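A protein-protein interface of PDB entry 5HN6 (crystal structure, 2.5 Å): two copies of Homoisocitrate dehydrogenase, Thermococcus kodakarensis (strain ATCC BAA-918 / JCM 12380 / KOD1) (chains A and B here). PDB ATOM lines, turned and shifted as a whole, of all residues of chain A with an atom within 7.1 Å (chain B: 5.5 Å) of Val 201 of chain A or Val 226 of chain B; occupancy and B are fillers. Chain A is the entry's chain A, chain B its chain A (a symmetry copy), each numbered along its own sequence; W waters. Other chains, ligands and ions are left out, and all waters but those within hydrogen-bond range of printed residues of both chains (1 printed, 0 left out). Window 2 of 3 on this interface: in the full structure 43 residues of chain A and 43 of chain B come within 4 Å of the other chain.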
ATOM      1  N   PHE A 196      29.784 -29.944 -17.695  1.00  0.00           N
ATOM      2  CA  PHE A 196      28.348 -29.891 -18.030  1.00  0.00           C
ATOM      3  C   PHE A 196      27.744 -28.534 -17.845  1.00  0.00           C
ATOM      4  O   PHE A 196      26.746 -28.234 -18.500  1.00  0.00           O
ATOM      5  CB  PHE A 196      27.520 -30.930 -17.286  1.00  0.00           C
ATOM      6  CG  PHE A 196      26.107 -31.045 -17.777  1.00  0.00           C
ATOM      7  CD1 PHE A 196      25.840 -31.595 -19.006  1.00  0.00           C
ATOM      8  CD2 PHE A 196      25.053 -30.636 -16.997  1.00  0.00           C
ATOM      9  CE1 PHE A 196      24.541 -31.720 -19.477  1.00  0.00           C
ATOM     10  CE2 PHE A 196      23.747 -30.764 -17.440  1.00  0.00           C
ATOM     11  CZ  PHE A 196      23.487 -31.282 -18.698  1.00  0.00           C
ATOM     12  N   THR A 197      28.327 -27.694 -16.990  1.00  0.00           N
ATOM     13  CA  THR A 197      27.830 -26.312 -16.879  1.00  0.00           C
ATOM     14  C   THR A 197      28.009 -25.605 -18.235  1.00  0.00           C
ATOM     15  O   THR A 197      27.171 -24.849 -18.667  1.00  0.00           O
ATOM     16  CB  THR A 197      28.539 -25.506 -15.771  1.00  0.00           C
ATOM     17  OG1 THR A 197      29.962 -25.514 -15.986  1.00  0.00           O
ATOM     18  CG2 THR A 197      28.230 -26.087 -14.416  1.00  0.00           C
ATOM     19  N   ILE A 198      29.115 -25.882 -18.912  1.00  0.00           N
ATOM     20  CA  ILE A 198      29.384 -25.275 -20.187  1.00  0.00           C
ATOM     21  C   ILE A 198      28.352 -25.781 -21.191  1.00  0.00           C
ATOM     22  O   ILE A 198      27.681 -24.975 -21.846  1.00  0.00           O
ATOM     23  CB  ILE A 198      30.816 -25.591 -20.672  1.00  0.00           C
ATOM     24  CG1 ILE A 198      31.851 -24.897 -19.785  1.00  0.00           C
ATOM     25  CG2 ILE A 198      31.009 -25.154 -22.125  1.00  0.00           C
ATOM     26  CD1 ILE A 198      33.270 -25.354 -20.069  1.00  0.00           C
ATOM     27  N   LYS A 199      28.218 -27.110 -21.305  1.00  0.00           N
ATOM     28  CA  LYS A 199      27.197 -27.693 -22.178  1.00  0.00           C
ATOM     29  C   LYS A 199      25.803 -27.155 -21.881  1.00  0.00           C
ATOM     30  O   LYS A 199      24.983 -27.010 -22.775  1.00  0.00           O
ATOM     31  CB  LYS A 199      27.205 -29.204 -22.085  1.00  0.00           C
ATOM     32  CG  LYS A 199      28.445 -29.864 -22.695  1.00  0.00           C
ATOM     33  CD  LYS A 199      28.330 -31.366 -22.632  1.00  0.00           C
ATOM     34  CE  LYS A 199      29.501 -32.061 -23.301  1.00  0.00           C
ATOM     35  NZ  LYS A 199      30.635 -32.176 -22.366  1.00  0.00           N
ATOM     36  N   LEU A 200      25.532 -26.829 -20.622  1.00  0.00           N
ATOM     37  CA  LEU A 200      24.180 -26.509 -20.244  1.00  0.00           C
ATOM     38  C   LEU A 200      23.833 -25.091 -20.634  1.00  0.00           C
ATOM     39  O   LEU A 200      22.656 -24.792 -20.919  1.00  0.00           O
ATOM     40  CB  LEU A 200      23.971 -26.738 -18.754  1.00  0.00           C
ATOM     41  CG  LEU A 200      22.559 -26.395 -18.253  1.00  0.00           C
ATOM     42  CD1 LEU A 200      21.506 -27.122 -19.077  1.00  0.00           C
ATOM     43  CD2 LEU A 200      22.403 -26.732 -16.779  1.00  0.00           C
ATOM     44  N   VAL A 201      24.819 -24.196 -20.642  1.00  0.00           N
ATOM     45  CA  VAL A 201      24.512 -22.859 -21.137  1.00  0.00           C
ATOM     46  C   VAL A 201      24.617 -22.743 -22.678  1.00  0.00           C
ATOM     47  O   VAL A 201      23.826 -22.045 -23.266  1.00  0.00           O
ATOM     48  CB  VAL A 201      25.213 -21.686 -20.407  1.00  0.00           C
ATOM     49  CG1 VAL A 201      25.795 -22.086 -19.075  1.00  0.00           C
ATOM     50  CG2 VAL A 201      26.198 -21.000 -21.309  1.00  0.00           C
ATOM     51  N   ARG A 202      25.570 -23.410 -23.316  1.00  0.00           N
ATOM     52  CA  ARG A 202      25.788 -23.260 -24.775  1.00  0.00           C
ATOM     53  C   ARG A 202      24.756 -24.082 -25.532  1.00  0.00           C
ATOM     54  O   ARG A 202      24.176 -23.634 -26.511  1.00  0.00           O
ATOM     55  CB  ARG A 202      27.165 -23.792 -25.201  1.00  0.00           C
ATOM     56  CG  ARG A 202      28.362 -23.079 -24.605  1.00  0.00           C
ATOM     57  CD  ARG A 202      28.880 -21.984 -25.524  1.00  0.00           C
ATOM     58  NE  ARG A 202      30.086 -21.379 -24.976  1.00  0.00           N
ATOM     59  CZ  ARG A 202      31.285 -21.947 -24.974  1.00  0.00           C
ATOM     60  NH1 ARG A 202      31.467 -23.145 -25.525  1.00  0.00           N
ATOM     61  NH2 ARG A 202      32.314 -21.301 -24.426  1.00  0.00           N
ATOM     62  N   ASN A 203      24.551 -25.303 -25.064  1.00  0.00           N
ATOM     63  CA  ASN A 203      23.713 -26.257 -25.729  1.00  0.00           C
ATOM     64  C   ASN A 203      22.552 -26.771 -24.858  1.00  0.00           C
ATOM     65  O   ASN A 203      22.505 -27.948 -24.507  1.00  0.00           O
ATOM     66  CB  ASN A 203      24.592 -27.432 -26.153  1.00  0.00           C
ATOM     67  CG  ASN A 203      23.883 -28.339 -27.116  1.00  0.00           C
ATOM     68  OD1 ASN A 203      22.820 -27.960 -27.656  1.00  0.00           O
ATOM     69  ND2 ASN A 203      24.424 -29.544 -27.336  1.00  0.00           N
ATOM     70  N   PRO A 204      21.586 -25.905 -24.545  1.00  0.00           N
ATOM     71  CA  PRO A 204      20.622 -26.278 -23.492  1.00  0.00           C
ATOM     72  C   PRO A 204      19.754 -27.514 -23.704  1.00  0.00           C
ATOM     73  O   PRO A 204      19.470 -28.199 -22.722  1.00  0.00           O
ATOM     74  CB  PRO A 204      19.738 -25.033 -23.342  1.00  0.00           C
ATOM     75  CG  PRO A 204      20.135 -24.083 -24.439  1.00  0.00           C
ATOM     76  CD  PRO A 204      21.518 -24.473 -24.877  1.00  0.00           C
ATOM     77  N   HIS A 207      19.931 -32.615 -23.837  1.00  0.00           N
ATOM     78  CA  HIS A 207      20.428 -33.443 -22.730  1.00  0.00           C
ATOM     79  C   HIS A 207      19.483 -34.439 -22.138  1.00  0.00           C
ATOM     80  O   HIS A 207      19.857 -35.200 -21.239  1.00  0.00           O
ATOM     81  CB  HIS A 207      20.976 -32.529 -21.667  1.00  0.00           C
ATOM     82  CG  HIS A 207      22.099 -31.701 -22.172  1.00  0.00           C
ATOM     83  ND1 HIS A 207      23.267 -32.265 -22.642  1.00  0.00           N
ATOM     84  CD2 HIS A 207      22.217 -30.366 -22.349  1.00  0.00           C
ATOM     85  CE1 HIS A 207      24.073 -31.303 -23.051  1.00  0.00           C
ATOM     86  NE2 HIS A 207      23.462 -30.142 -22.876  1.00  0.00           N
ATOM     87  N   LEU A 223      21.069 -22.875 -12.504  1.00  0.00           N
ATOM     88  CA  LEU A 223      21.774 -22.481 -13.713  1.00  0.00           C
ATOM     89  C   LEU A 223      20.899 -22.585 -14.965  1.00  0.00           C
ATOM     90  O   LEU A 223      20.995 -21.744 -15.864  1.00  0.00           O
ATOM     91  CB  LEU A 223      23.027 -23.331 -13.924  1.00  0.00           C
ATOM     92  CG  LEU A 223      23.776 -23.162 -15.251  1.00  0.00           C
ATOM     93  CD1 LEU A 223      24.207 -21.726 -15.439  1.00  0.00           C
ATOM     94  CD2 LEU A 223      24.998 -24.056 -15.288  1.00  0.00           C
ATOM     95  N   ALA A 224      20.078 -23.631 -15.051  1.00  0.00           N
ATOM     96  CA  ALA A 224      19.304 -23.861 -16.275  1.00  0.00           C
ATOM     97  C   ALA A 224      18.257 -22.784 -16.516  1.00  0.00           C
ATOM     98  O   ALA A 224      17.763 -22.660 -17.624  1.00  0.00           O
ATOM     99  CB  ALA A 224      18.640 -25.225 -16.256  1.00  0.00           C
ATOM    100  N   VAL A 226      18.770 -19.674 -16.701  1.00  0.00           N
ATOM    101  CA  VAL A 226      19.213 -18.644 -17.625  1.00  0.00           C
ATOM    102  C   VAL A 226      18.465 -18.768 -18.962  1.00  0.00           C
ATOM    103  O   VAL A 226      18.289 -17.769 -19.637  1.00  0.00           O
ATOM    104  CB  VAL A 226      20.730 -18.644 -17.891  1.00  0.00           C
ATOM    105  CG1 VAL A 226      21.487 -18.351 -16.625  1.00  0.00           C
ATOM    106  CG2 VAL A 226      21.189 -19.920 -18.595  1.00  0.00           C
ATOM    107  N   HIS A 227      18.023 -19.976 -19.323  1.00  0.00           N
ATOM    108  CA  HIS A 227      17.337 -20.211 -20.603  1.00  0.00           C
ATOM    109  C   HIS A 227      15.834 -19.883 -20.670  1.00  0.00           C
ATOM    110  O   HIS A 227      15.306 -19.576 -21.737  1.00  0.00           O
ATOM    111  CB  HIS A 227      17.528 -21.635 -21.030  1.00  0.00           C
ATOM    112  CG  HIS A 227      18.959 -22.003 -21.213  1.00  0.00           C
ATOM    113  ND1 HIS A 227      19.801 -21.301 -22.041  1.00  0.00           N
ATOM    114  CD2 HIS A 227      19.698 -23.001 -20.677  1.00  0.00           C
ATOM    115  CE1 HIS A 227      21.000 -21.847 -22.011  1.00  0.00           C
ATOM    116  NE2 HIS A 227      20.963 -22.885 -21.193  1.00  0.00           N
ATOM    117  N   VAL B 201      26.657 -16.093 -15.067  1.00  0.00           N
ATOM    118  CA  VAL B 201      26.469 -15.984 -16.508  1.00  0.00           C
ATOM    119  C   VAL B 201      25.860 -14.628 -16.941  1.00  0.00           C
ATOM    120  O   VAL B 201      26.238 -14.120 -17.970  1.00  0.00           O
ATOM    121  CB  VAL B 201      25.779 -17.189 -17.196  1.00  0.00           C
ATOM    122  CG1 VAL B 201      25.757 -18.426 -16.334  1.00  0.00           C
ATOM    123  CG2 VAL B 201      24.428 -16.806 -17.728  1.00  0.00           C
ATOM    124  N   ASP B 222      34.930 -23.705 -14.645  1.00  0.00           N
ATOM    125  CA  ASP B 222      34.520 -24.175 -15.944  1.00  0.00           C
ATOM    126  C   ASP B 222      33.355 -23.335 -16.421  1.00  0.00           C
ATOM    127  O   ASP B 222      33.357 -22.878 -17.558  1.00  0.00           O
ATOM    128  CB  ASP B 222      34.066 -25.609 -15.879  1.00  0.00           C
ATOM    129  CG  ASP B 222      35.126 -26.568 -16.265  1.00  0.00           C
ATOM    130  OD1 ASP B 222      36.313 -26.365 -15.909  1.00  0.00           O
ATOM    131  OD2 ASP B 222      34.736 -27.563 -16.908  1.00  0.00           O
ATOM    132  N   LEU B 223      32.359 -23.112 -15.567  1.00  0.00           N
ATOM    133  CA  LEU B 223      31.237 -22.289 -15.989  1.00  0.00           C
ATOM    134  C   LEU B 223      31.672 -20.899 -16.460  1.00  0.00           C
ATOM    135  O   LEU B 223      31.103 -20.358 -17.414  1.00  0.00           O
ATOM    136  CB  LEU B 223      30.219 -22.124 -14.861  1.00  0.00           C
ATOM    137  CG  LEU B 223      29.072 -21.131 -15.090  1.00  0.00           C
ATOM    138  CD1 LEU B 223      28.279 -21.510 -16.319  1.00  0.00           C
ATOM    139  CD2 LEU B 223      28.147 -21.104 -13.891  1.00  0.00           C
ATOM    140  N   ALA B 224      32.646 -20.299 -15.777  1.00  0.00           N
ATOM    141  CA  ALA B 224      33.026 -18.918 -16.095  1.00  0.00           C
ATOM    142  C   ALA B 224      33.659 -18.789 -17.472  1.00  0.00           C
ATOM    143  O   ALA B 224      33.735 -17.692 -18.000  1.00  0.00           O
ATOM    144  CB  ALA B 224      33.963 -18.352 -15.045  1.00  0.00           C
ATOM    145  N   THR B 225      34.100 -19.906 -18.050  1.00  0.00           N
ATOM    146  CA  THR B 225      34.690 -19.900 -19.385  1.00  0.00           C
ATOM    147  C   THR B 225      33.692 -19.741 -20.510  1.00  0.00           C
ATOM    148  O   THR B 225      34.089 -19.675 -21.659  1.00  0.00           O
ATOM    149  CB  THR B 225      35.455 -21.196 -19.693  1.00  0.00           C
ATOM    150  OG1 THR B 225      34.524 -22.267 -20.010  1.00  0.00           O
ATOM    151  CG2 THR B 225      36.379 -21.564 -18.539  1.00  0.00           C
ATOM    152  N   VAL B 226      32.398 -19.714 -20.214  1.00  0.00           N
ATOM    153  CA  VAL B 226      31.457 -19.291 -21.237  1.00  0.00           C
ATOM    154  C   VAL B 226      31.753 -17.847 -21.671  1.00  0.00           C
ATOM    155  O   VAL B 226      31.467 -17.498 -22.803  1.00  0.00           O
ATOM    156  CB  VAL B 226      29.979 -19.404 -20.822  1.00  0.00           C
ATOM    157  CG1 VAL B 226      29.613 -20.838 -20.557  1.00  0.00           C
ATOM    158  CG2 VAL B 226      29.635 -18.464 -19.667  1.00  0.00           C
ATOM    159  N   HIS B 227      32.330 -17.032 -20.784  1.00  0.00           N
ATOM    160  CA  HIS B 227      32.612 -15.620 -21.082  1.00  0.00           C
ATOM    161  C   HIS B 227      33.896 -15.307 -21.872  1.00  0.00           C
ATOM    162  O   HIS B 227      33.972 -14.298 -22.570  1.00  0.00           O
ATOM    163  CB  HIS B 227      32.636 -14.824 -19.811  1.00  0.00           C
ATOM    164  CG  HIS B 227      31.350 -14.878 -19.063  1.00  0.00           C
ATOM    165  ND1 HIS B 227      30.150 -14.534 -19.637  1.00  0.00           N
ATOM    166  CD2 HIS B 227      31.074 -15.231 -17.788  1.00  0.00           C
ATOM    167  CE1 HIS B 227      29.185 -14.672 -18.750  1.00  0.00           C
ATOM    168  NE2 HIS B 227      29.720 -15.091 -17.616  1.00  0.00           N
ATOM    169  N   ALA B 228      34.917 -16.136 -21.726  1.00  0.00           N
ATOM    170  CA  ALA B 228      35.993 -16.140 -22.687  1.00  0.00           C
ATOM    171  C   ALA B 228      35.406 -16.942 -23.813  1.00  0.00           C
ATOM    172  O   ALA B 228      34.361 -17.571 -23.646  1.00  0.00           O
ATOM    173  CB  ALA B 228      37.217 -16.823 -22.131  1.00  0.00           C
ATOM    174  N   GLY B 229      36.049 -16.973 -24.958  1.00  0.00           N
ATOM    175  CA  GLY B 229      35.408 -17.673 -26.088  1.00  0.00           C
ATOM    176  C   GLY B 229      35.376 -19.190 -25.946  1.00  0.00           C
ATOM    177  O   GLY B 229      34.593 -19.875 -26.592  1.00  0.00           O
HETATM  178  O   HOH W   1      33.619 -22.623 -22.285  1.00  0.00           O
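Printed residues of chain B within 4 Å of Val 201 of chain A: Leu 223 (3.8 Å) and Val 226 (3.5 Å). His 207 of chain A touches none of the printed residues of chain B. Ala 224 of chain A touches none of the printed residues of chain B. Of the printed residues of chain B, Val 226 of chain A touches Val 201. Printed residues of chain A within 4 Å of Leu 223 of chain B: Thr 197 (3.4 Å) and Val 201 (3.8 Å). The nearest residue of chain B that does not touch Val 201 of chain A is Val 201 of chain B (4.6 Å). The nearest residue of chain A that does not touch Val 226 of chain B is Ile 198 of chain A (4.5 Å). The nearest printed residue of chain A that does not touch Asp 222 of chain B is Thr 197 of chain A (4.1 Å).
The side-chain hydroxyl of Thr 197 of chain A is in hydrogen-bond range of the backbone NH of Leu 223 of chain B (3.4 Å). NH2 of Arg 202 of chain A lies within hydrogen-bond range of O of Gly 229 of chain B (3.5 Å).
Val 201 of chain A touches Leu 223 of chain B, and with the chains exchanged Leu 223 of chain A touches Val 201 of chain B. Val 201 of chain A touches Val 226 of chain B, and with the chains exchanged Val 226 of chain A touches Val 201 of chain B. Of the 10 pairs that touch across the chains among the printed residues, 4 have their exchanged pair printed and touching as well.
Printed residues of chain A that touch a printed residue of chain B: Thr 197, Ile 198, Val 201, Arg 202, Leu 223 and Val 226. Hydrophobic or aromatic side chains of chain A that line the printed part of chain B: Ile 198, Val 201, Leu 223 and Val 226. Among the printed residues, 10 pairs touch across the chains. Among the printed residues, no Asp or Glu carboxylate lies within 4 Å of a Lys or Arg side-chain nitrogen of the other chain.
Water W1 bridges the side-chain hydroxyl of Thr 225 of chain B (2.5 Å) and the guanidinium group of Arg 202 of chain A (2.8 Å).
The backbone carbonyl oxygen of Asp 222 of chain B is in hydrogen-bond range of the side-chain hydroxyl of Thr 225 of chain B, 2.8 Å away.
Among the printed residues, pairs that only touch across the chains: Ile 198 of chain A with Thr 225 of chain B (3.3 Å), Ile 198 of chain A with Asp 222 of chain B (3.4 Å), Val 226 of chain A with Val 201 of chain B (3.5 Å), Val 201 of chain A with Val 226 of chain B (3.5 Å), Arg 202 of chain A with Thr 225 of chain B (3.7 Å), Leu 223 of chain A with Val 201 of chain B (3.8 Å), Val 201 of chain A with Leu 223 of chain B (3.8 Å) and Arg 202 of chain A with Val 226 of chain B (3.9 Å).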
